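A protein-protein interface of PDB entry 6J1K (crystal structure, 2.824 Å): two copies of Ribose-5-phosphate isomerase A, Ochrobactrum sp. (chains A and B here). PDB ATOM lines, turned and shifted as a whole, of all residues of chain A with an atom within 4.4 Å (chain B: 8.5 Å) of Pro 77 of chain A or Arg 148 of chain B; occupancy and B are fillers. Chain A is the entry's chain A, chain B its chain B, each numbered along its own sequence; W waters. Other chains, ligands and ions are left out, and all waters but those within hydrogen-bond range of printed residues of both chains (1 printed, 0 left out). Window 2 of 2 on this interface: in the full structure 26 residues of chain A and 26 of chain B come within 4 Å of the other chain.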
ATOM      1  N   LEU A  73      31.164 -24.359  18.036  1.00  0.00           N
ATOM      2  CA  LEU A  73      30.523 -25.028  16.901  1.00  0.00           C
ATOM      3  C   LEU A  73      29.657 -24.077  16.062  1.00  0.00           C
ATOM      4  O   LEU A  73      29.447 -24.331  14.871  1.00  0.00           O
ATOM      5  CB  LEU A  73      29.712 -26.240  17.359  1.00  0.00           C
ATOM      6  CG  LEU A  73      30.565 -27.474  17.694  1.00  0.00           C
ATOM      7  CD1 LEU A  73      29.757 -28.406  18.566  1.00  0.00           C
ATOM      8  CD2 LEU A  73      31.105 -28.191  16.441  1.00  0.00           C
ATOM      9  N   ASP A  74      29.145 -22.990  16.644  1.00  0.00           N
ATOM     10  CA  ASP A  74      28.517 -21.946  15.838  1.00  0.00           C
ATOM     11  C   ASP A  74      29.536 -21.307  14.907  1.00  0.00           C
ATOM     12  O   ASP A  74      29.219 -20.994  13.756  1.00  0.00           O
ATOM     13  CB  ASP A  74      27.890 -20.886  16.733  1.00  0.00           C
ATOM     14  CG  ASP A  74      26.963 -21.480  17.743  1.00  0.00           C
ATOM     15  OD1 ASP A  74      26.073 -22.250  17.332  1.00  0.00           O
ATOM     16  OD2 ASP A  74      27.163 -21.217  18.947  1.00  0.00           O
ATOM     17  N   GLU A  75      30.756 -21.060  15.405  1.00  0.00           N
ATOM     18  CA  GLU A  75      31.834 -20.516  14.579  1.00  0.00           C
ATOM     19  C   GLU A  75      32.574 -21.572  13.761  1.00  0.00           C
ATOM     20  O   GLU A  75      32.993 -21.290  12.632  1.00  0.00           O
ATOM     21  CB  GLU A  75      32.856 -19.786  15.462  1.00  0.00           C
ATOM     22  CG  GLU A  75      32.478 -18.360  15.824  1.00  0.00           C
ATOM     23  CD  GLU A  75      31.456 -18.305  16.942  1.00  0.00           C
ATOM     24  OE1 GLU A  75      30.242 -18.204  16.634  1.00  0.00           O
ATOM     25  OE2 GLU A  75      31.876 -18.346  18.126  1.00  0.00           O
ATOM     26  N   THR A  76      32.705 -22.792  14.284  1.00  0.00           N
ATOM     27  CA  THR A  76      33.515 -23.856  13.674  1.00  0.00           C
ATOM     28  C   THR A  76      32.675 -25.135  13.682  1.00  0.00           C
ATOM     29  O   THR A  76      32.831 -26.010  14.548  1.00  0.00           O
ATOM     30  CB  THR A  76      34.848 -24.020  14.419  1.00  0.00           C
ATOM     31  OG1 THR A  76      35.514 -22.754  14.489  1.00  0.00           O
ATOM     32  CG2 THR A  76      35.759 -25.012  13.713  1.00  0.00           C
ATOM     33  N   PRO A  77      31.711 -25.241  12.753  1.00  0.00           N
ATOM     34  CA  PRO A  77      30.668 -26.266  12.889  1.00  0.00           C
ATOM     35  C   PRO A  77      31.093 -27.675  12.547  1.00  0.00           C
ATOM     36  O   PRO A  77      30.367 -28.618  12.892  1.00  0.00           O
ATOM     37  CB  PRO A  77      29.558 -25.780  11.936  1.00  0.00           C
ATOM     38  CG  PRO A  77      29.969 -24.418  11.487  1.00  0.00           C
ATOM     39  CD  PRO A  77      31.460 -24.372  11.593  1.00  0.00           C
ATOM     40  N   HIS A  78      32.195 -27.867  11.850  1.00  0.00           N
ATOM     41  CA  HIS A  78      32.691 -29.211  11.596  1.00  0.00           C
ATOM     42  C   HIS A  78      34.125 -29.306  12.081  1.00  0.00           C
ATOM     43  O   HIS A  78      34.921 -28.376  11.906  1.00  0.00           O
ATOM     44  CB  HIS A  78      32.581 -29.604  10.123  1.00  0.00           C
ATOM     45  CG  HIS A  78      32.868 -31.050   9.857  1.00  0.00           C
ATOM     46  ND1 HIS A  78      32.010 -32.066  10.219  1.00  0.00           N
ATOM     47  CD2 HIS A  78      33.922 -31.649   9.254  1.00  0.00           C
ATOM     48  CE1 HIS A  78      32.513 -33.227   9.838  1.00  0.00           C
ATOM     49  NE2 HIS A  78      33.675 -33.002   9.253  1.00  0.00           N
ATOM     50  N   LEU A  79      34.427 -30.411  12.735  1.00  0.00           N
ATOM     51  CA  LEU A  79      35.739 -30.659  13.287  1.00  0.00           C
ATOM     52  C   LEU A  79      36.367 -31.869  12.608  1.00  0.00           C
ATOM     53  O   LEU A  79      35.690 -32.678  11.960  1.00  0.00           O
ATOM     54  CB  LEU A  79      35.633 -30.876  14.790  1.00  0.00           C
ATOM     55  CG  LEU A  79      35.118 -29.682  15.588  1.00  0.00           C
ATOM     56  CD1 LEU A  79      34.252 -30.121  16.768  1.00  0.00           C
ATOM     57  CD2 LEU A  79      36.337 -28.952  16.055  1.00  0.00           C
ATOM     58  N   ALA A 112      29.871 -34.206  15.255  1.00  0.00           N
ATOM     59  CA  ALA A 112      30.326 -33.195  14.303  1.00  0.00           C
ATOM     60  C   ALA A 112      31.758 -33.417  13.819  1.00  0.00           C
ATOM     61  O   ALA A 112      32.326 -32.519  13.188  1.00  0.00           O
ATOM     62  CB  ALA A 112      30.193 -31.796  14.905  1.00  0.00           C
ATOM     63  N   GLY B 142      26.116 -25.852  20.162  1.00  0.00           N
ATOM     64  CA  GLY B 142      26.365 -26.520  18.890  1.00  0.00           C
ATOM     65  C   GLY B 142      25.302 -26.362  17.822  1.00  0.00           C
ATOM     66  O   GLY B 142      25.221 -27.207  16.923  1.00  0.00           O
ATOM     67  N   LEU B 143      24.512 -25.279  17.862  1.00  0.00           N
ATOM     68  CA  LEU B 143      23.476 -25.046  16.851  1.00  0.00           C
ATOM     69  C   LEU B 143      24.003 -25.153  15.422  1.00  0.00           C
ATOM     70  O   LEU B 143      23.378 -25.786  14.569  1.00  0.00           O
ATOM     71  CB  LEU B 143      22.817 -23.687  17.062  1.00  0.00           C
ATOM     72  CG  LEU B 143      21.617 -23.306  16.174  1.00  0.00           C
ATOM     73  CD1 LEU B 143      20.458 -24.169  16.534  1.00  0.00           C
ATOM     74  CD2 LEU B 143      21.222 -21.810  16.307  1.00  0.00           C
ATOM     75  N   GLY B 144      25.157 -24.565  15.137  1.00  0.00           N
ATOM     76  CA  GLY B 144      25.664 -24.665  13.776  1.00  0.00           C
ATOM     77  C   GLY B 144      25.828 -26.085  13.273  1.00  0.00           C
ATOM     78  O   GLY B 144      25.362 -26.418  12.176  1.00  0.00           O
ATOM     79  N   ALA B 145      26.453 -26.946  14.075  1.00  0.00           N
ATOM     80  CA  ALA B 145      26.628 -28.319  13.631  1.00  0.00           C
ATOM     81  C   ALA B 145      25.278 -29.033  13.555  1.00  0.00           C
ATOM     82  O   ALA B 145      25.101 -29.951  12.742  1.00  0.00           O
ATOM     83  CB  ALA B 145      27.605 -29.052  14.548  1.00  0.00           C
ATOM     84  N   THR B 146      24.339 -28.664  14.437  1.00  0.00           N
ATOM     85  CA  THR B 146      23.005 -29.260  14.406  1.00  0.00           C
ATOM     86  C   THR B 146      22.229 -28.888  13.139  1.00  0.00           C
ATOM     87  O   THR B 146      21.479 -29.721  12.602  1.00  0.00           O
ATOM     88  CB  THR B 146      22.261 -28.897  15.685  1.00  0.00           C
ATOM     89  OG1 THR B 146      22.942 -29.526  16.780  1.00  0.00           O
ATOM     90  CG2 THR B 146      20.826 -29.397  15.665  1.00  0.00           C
ATOM     91  N   MET B 147      22.375 -27.640  12.663  1.00  0.00           N
ATOM     92  CA  MET B 147      21.788 -27.249  11.377  1.00  0.00           C
ATOM     93  C   MET B 147      22.342 -28.101  10.241  1.00  0.00           C
ATOM     94  O   MET B 147      21.587 -28.611   9.410  1.00  0.00           O
ATOM     95  CB  MET B 147      22.068 -25.780  11.078  1.00  0.00           C
ATOM     96  CG  MET B 147      21.884 -24.825  12.217  1.00  0.00           C
ATOM     97  SD  MET B 147      20.198 -24.306  12.332  1.00  0.00           S
ATOM     98  CE  MET B 147      20.176 -23.034  11.048  1.00  0.00           C
ATOM     99  N   ARG B 148      23.672 -28.260  10.183  1.00  0.00           N
ATOM    100  CA  ARG B 148      24.269 -29.111   9.153  1.00  0.00           C
ATOM    101  C   ARG B 148      23.648 -30.493   9.187  1.00  0.00           C
ATOM    102  O   ARG B 148      23.170 -30.996   8.169  1.00  0.00           O
ATOM    103  CB  ARG B 148      25.778 -29.248   9.352  1.00  0.00           C
ATOM    104  CG  ARG B 148      26.593 -28.003   9.170  1.00  0.00           C
ATOM    105  CD  ARG B 148      27.251 -27.925   7.807  1.00  0.00           C
ATOM    106  NE  ARG B 148      28.040 -26.696   7.747  1.00  0.00           N
ATOM    107  CZ  ARG B 148      29.305 -26.598   8.159  1.00  0.00           C
ATOM    108  NH1 ARG B 148      29.945 -27.662   8.644  1.00  0.00           N
ATOM    109  NH2 ARG B 148      29.927 -25.429   8.102  1.00  0.00           N
ATOM    110  N   ALA B 149      23.582 -31.080  10.383  1.00  0.00           N
ATOM    111  CA  ALA B 149      23.095 -32.445  10.559  1.00  0.00           C
ATOM    112  C   ALA B 149      21.626 -32.586  10.176  1.00  0.00           C
ATOM    113  O   ALA B 149      21.195 -33.646   9.696  1.00  0.00           O
ATOM    114  CB  ALA B 149      23.305 -32.883  12.003  1.00  0.00           C
ATOM    115  N   ILE B 150      20.826 -31.558  10.440  1.00  0.00           N
ATOM    116  CA  ILE B 150      19.438 -31.621  10.013  1.00  0.00           C
ATOM    117  C   ILE B 150      19.331 -31.643   8.490  1.00  0.00           C
ATOM    118  O   ILE B 150      18.496 -32.368   7.937  1.00  0.00           O
ATOM    119  CB  ILE B 150      18.624 -30.469  10.626  1.00  0.00           C
ATOM    120  CG1 ILE B 150      18.420 -30.669  12.129  1.00  0.00           C
ATOM    121  CG2 ILE B 150      17.294 -30.368   9.944  1.00  0.00           C
ATOM    122  CD1 ILE B 150      17.837 -29.463  12.808  1.00  0.00           C
ATOM    123  N   GLU B 151      20.170 -30.864   7.784  1.00  0.00           N
ATOM    124  CA  GLU B 151      20.103 -30.888   6.326  1.00  0.00           C
ATOM    125  C   GLU B 151      20.566 -32.244   5.794  1.00  0.00           C
ATOM    126  O   GLU B 151      19.893 -32.839   4.941  1.00  0.00           O
ATOM    127  CB  GLU B 151      20.931 -29.726   5.744  1.00  0.00           C
ATOM    128  CG  GLU B 151      21.002 -29.628   4.199  1.00  0.00           C
ATOM    129  CD  GLU B 151      22.000 -30.634   3.570  1.00  0.00           C
ATOM    130  OE1 GLU B 151      23.030 -30.974   4.207  1.00  0.00           O
ATOM    131  OE2 GLU B 151      21.731 -31.136   2.449  1.00  0.00           O
ATOM    132  N   GLU B 152      21.649 -32.796   6.369  1.00  0.00           N
ATOM    133  CA  GLU B 152      22.131 -34.113   5.963  1.00  0.00           C
ATOM    134  C   GLU B 152      21.143 -35.197   6.351  1.00  0.00           C
ATOM    135  O   GLU B 152      20.882 -36.095   5.551  1.00  0.00           O
ATOM    136  CB  GLU B 152      23.512 -34.392   6.566  1.00  0.00           C
ATOM    137  CG  GLU B 152      24.470 -33.206   6.421  1.00  0.00           C
ATOM    138  CD  GLU B 152      25.953 -33.558   6.518  1.00  0.00           C
ATOM    139  OE1 GLU B 152      26.592 -33.182   7.540  1.00  0.00           O
ATOM    140  OE2 GLU B 152      26.473 -34.188   5.573  1.00  0.00           O
ATOM    141  N   ALA B 153      20.534 -35.109   7.542  1.00  0.00           N
ATOM    142  CA  ALA B 153      19.466 -36.065   7.860  1.00  0.00           C
ATOM    143  C   ALA B 153      18.328 -35.980   6.842  1.00  0.00           C
ATOM    144  O   ALA B 153      17.788 -37.010   6.413  1.00  0.00           O
ATOM    145  CB  ALA B 153      18.932 -35.877   9.278  1.00  0.00           C
ATOM    146  N   ALA B 154      17.933 -34.759   6.460  1.00  0.00           N
ATOM    147  CA  ALA B 154      16.878 -34.603   5.464  1.00  0.00           C
ATOM    148  C   ALA B 154      17.301 -35.194   4.132  1.00  0.00           C
ATOM    149  O   ALA B 154      16.541 -35.933   3.499  1.00  0.00           O
ATOM    150  CB  ALA B 154      16.511 -33.132   5.290  1.00  0.00           C
ATOM    151  N   ALA B 155      18.516 -34.873   3.685  1.00  0.00           N
ATOM    152  CA  ALA B 155      18.979 -35.375   2.395  1.00  0.00           C
ATOM    153  C   ALA B 155      18.901 -36.886   2.337  1.00  0.00           C
ATOM    154  O   ALA B 155      18.405 -37.450   1.354  1.00  0.00           O
ATOM    155  CB  ALA B 155      20.405 -34.909   2.135  1.00  0.00           C
ATOM    156  N   LYS B 156      19.285 -37.550   3.430  1.00  0.00           N
ATOM    157  CA  LYS B 156      19.334 -39.011   3.450  1.00  0.00           C
ATOM    158  C   LYS B 156      17.957 -39.638   3.350  1.00  0.00           C
ATOM    159  O   LYS B 156      17.838 -40.788   2.933  1.00  0.00           O
ATOM    160  CB  LYS B 156      20.030 -39.509   4.718  1.00  0.00           C
ATOM    161  CG  LYS B 156      21.448 -39.041   4.880  1.00  0.00           C
ATOM    162  CD  LYS B 156      22.163 -39.837   5.966  1.00  0.00           C
ATOM    163  CE  LYS B 156      21.991 -39.211   7.337  1.00  0.00           C
ATOM    164  NZ  LYS B 156      23.068 -39.662   8.273  1.00  0.00           N
ATOM    165  N   LEU B 163      15.988 -24.233   6.685  1.00  0.00           N
ATOM    166  CA  LEU B 163      15.898 -24.338   8.141  1.00  0.00           C
ATOM    167  C   LEU B 163      16.014 -22.943   8.749  1.00  0.00           C
ATOM    168  O   LEU B 163      17.088 -22.331   8.683  1.00  0.00           O
ATOM    169  CB  LEU B 163      17.023 -25.226   8.681  1.00  0.00           C
ATOM    170  CG  LEU B 163      17.266 -26.506   7.892  1.00  0.00           C
ATOM    171  CD1 LEU B 163      18.401 -27.265   8.549  1.00  0.00           C
ATOM    172  CD2 LEU B 163      15.996 -27.346   7.795  1.00  0.00           C
ATOM    173  N   ILE B 202      20.590 -37.285  15.596  1.00  0.00           N
ATOM    174  CA  ILE B 202      21.388 -36.081  15.783  1.00  0.00           C
ATOM    175  C   ILE B 202      21.410 -35.799  17.278  1.00  0.00           C
ATOM    176  O   ILE B 202      20.339 -35.731  17.892  1.00  0.00           O
ATOM    177  CB  ILE B 202      20.825 -34.894  14.984  1.00  0.00           C
ATOM    178  CG1 ILE B 202      20.729 -35.237  13.515  1.00  0.00           C
ATOM    179  CG2 ILE B 202      21.730 -33.683  15.066  1.00  0.00           C
ATOM    180  CD1 ILE B 202      19.827 -34.323  12.769  1.00  0.00           C
HETATM  181  O   HOH W   1      28.298 -23.641  20.642  1.00  0.00           O
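The backbone NH of Leu 79 of chain A is in hydrogen-bond range of the backbone carbonyl oxygen of Ala 112 of chain A, at 3.0 Å.
O of Gly 142 of chain B is in hydrogen-bond range of OG1 of Thr 146 of chain B.
ND1 of His 78 of chain A lies within hydrogen-bond range of O of Ala 112 of chain A (3.0 Å).
Printed residues of chain A that touch a printed residue of chain B: Leu 73, Asp 74, Pro 77, His 78 and Ala 112.
Of the 17 printed residues of chain B, 5 touch a printed residue of chain A.
Hydrophobic or aromatic side chains of chain B within 4 Å of the printed part of chain A: Leu 143 and Ala 145.
Along chain B the printed residues that touch a printed residue of chain A span positions 142 to 148.
Among the printed residues, 9 pairs touch across the chains.
Water W1 bridges the backbone NH (N) of Gly 142 of chain B (3.1 Å) and the side-chain carboxylate (OD2) of Asp 74 of chain A (3.2 Å).
No position is printed for both chains.
OD1 of Asp 74 of chain A sits at hydrogen-bond distance from N of Leu 143 of chain B, 3.4 Å away.
The side-chain carboxylate (OD1) of Asp 74 of chain A lies within hydrogen-bond range of the backbone NH (N) of Gly 144 of chain B (3.3 Å).
Arg 148 of chain B touches two residues of chain A.
Printed residues of chain B within 4 Å of Asp 74 of chain A: Leu 143 (3.4 Å) and Gly 144 (3.3 Å).
Of the printed residues of chain A, Gly 144 of chain B touches Leu 73 (3.95 Å), Asp 74 (3.3 Å) and Pro 77 (3.97 Å).
The nearest printed residue of chain A that does not touch Arg 148 of chain B is Thr 76 of chain A (6.2 Å).
The nearest printed residue of chain A that does not touch Gly 144 of chain B is Glu 75 of chain A (6.4 Å).
Among the printed residues, merely in contact across the chains: Leu 73 of chain A with Gly 142 of chain B (3.7 Å), Leu 73 of chain A with Gly 144 of chain B (3.95 Å), Pro 77 of chain A with Gly 144 of chain B (3.97 Å), Pro 77 of chain A with Ala 145 of chain B (3.2 Å), Pro 77 of chain A with Arg 148 of chain B (3.5 Å), His 78 of chain A with Arg 148 of chain B (3.6 Å) and Ala 112 of chain A with Ala 145 of chain B (3.8 Å).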
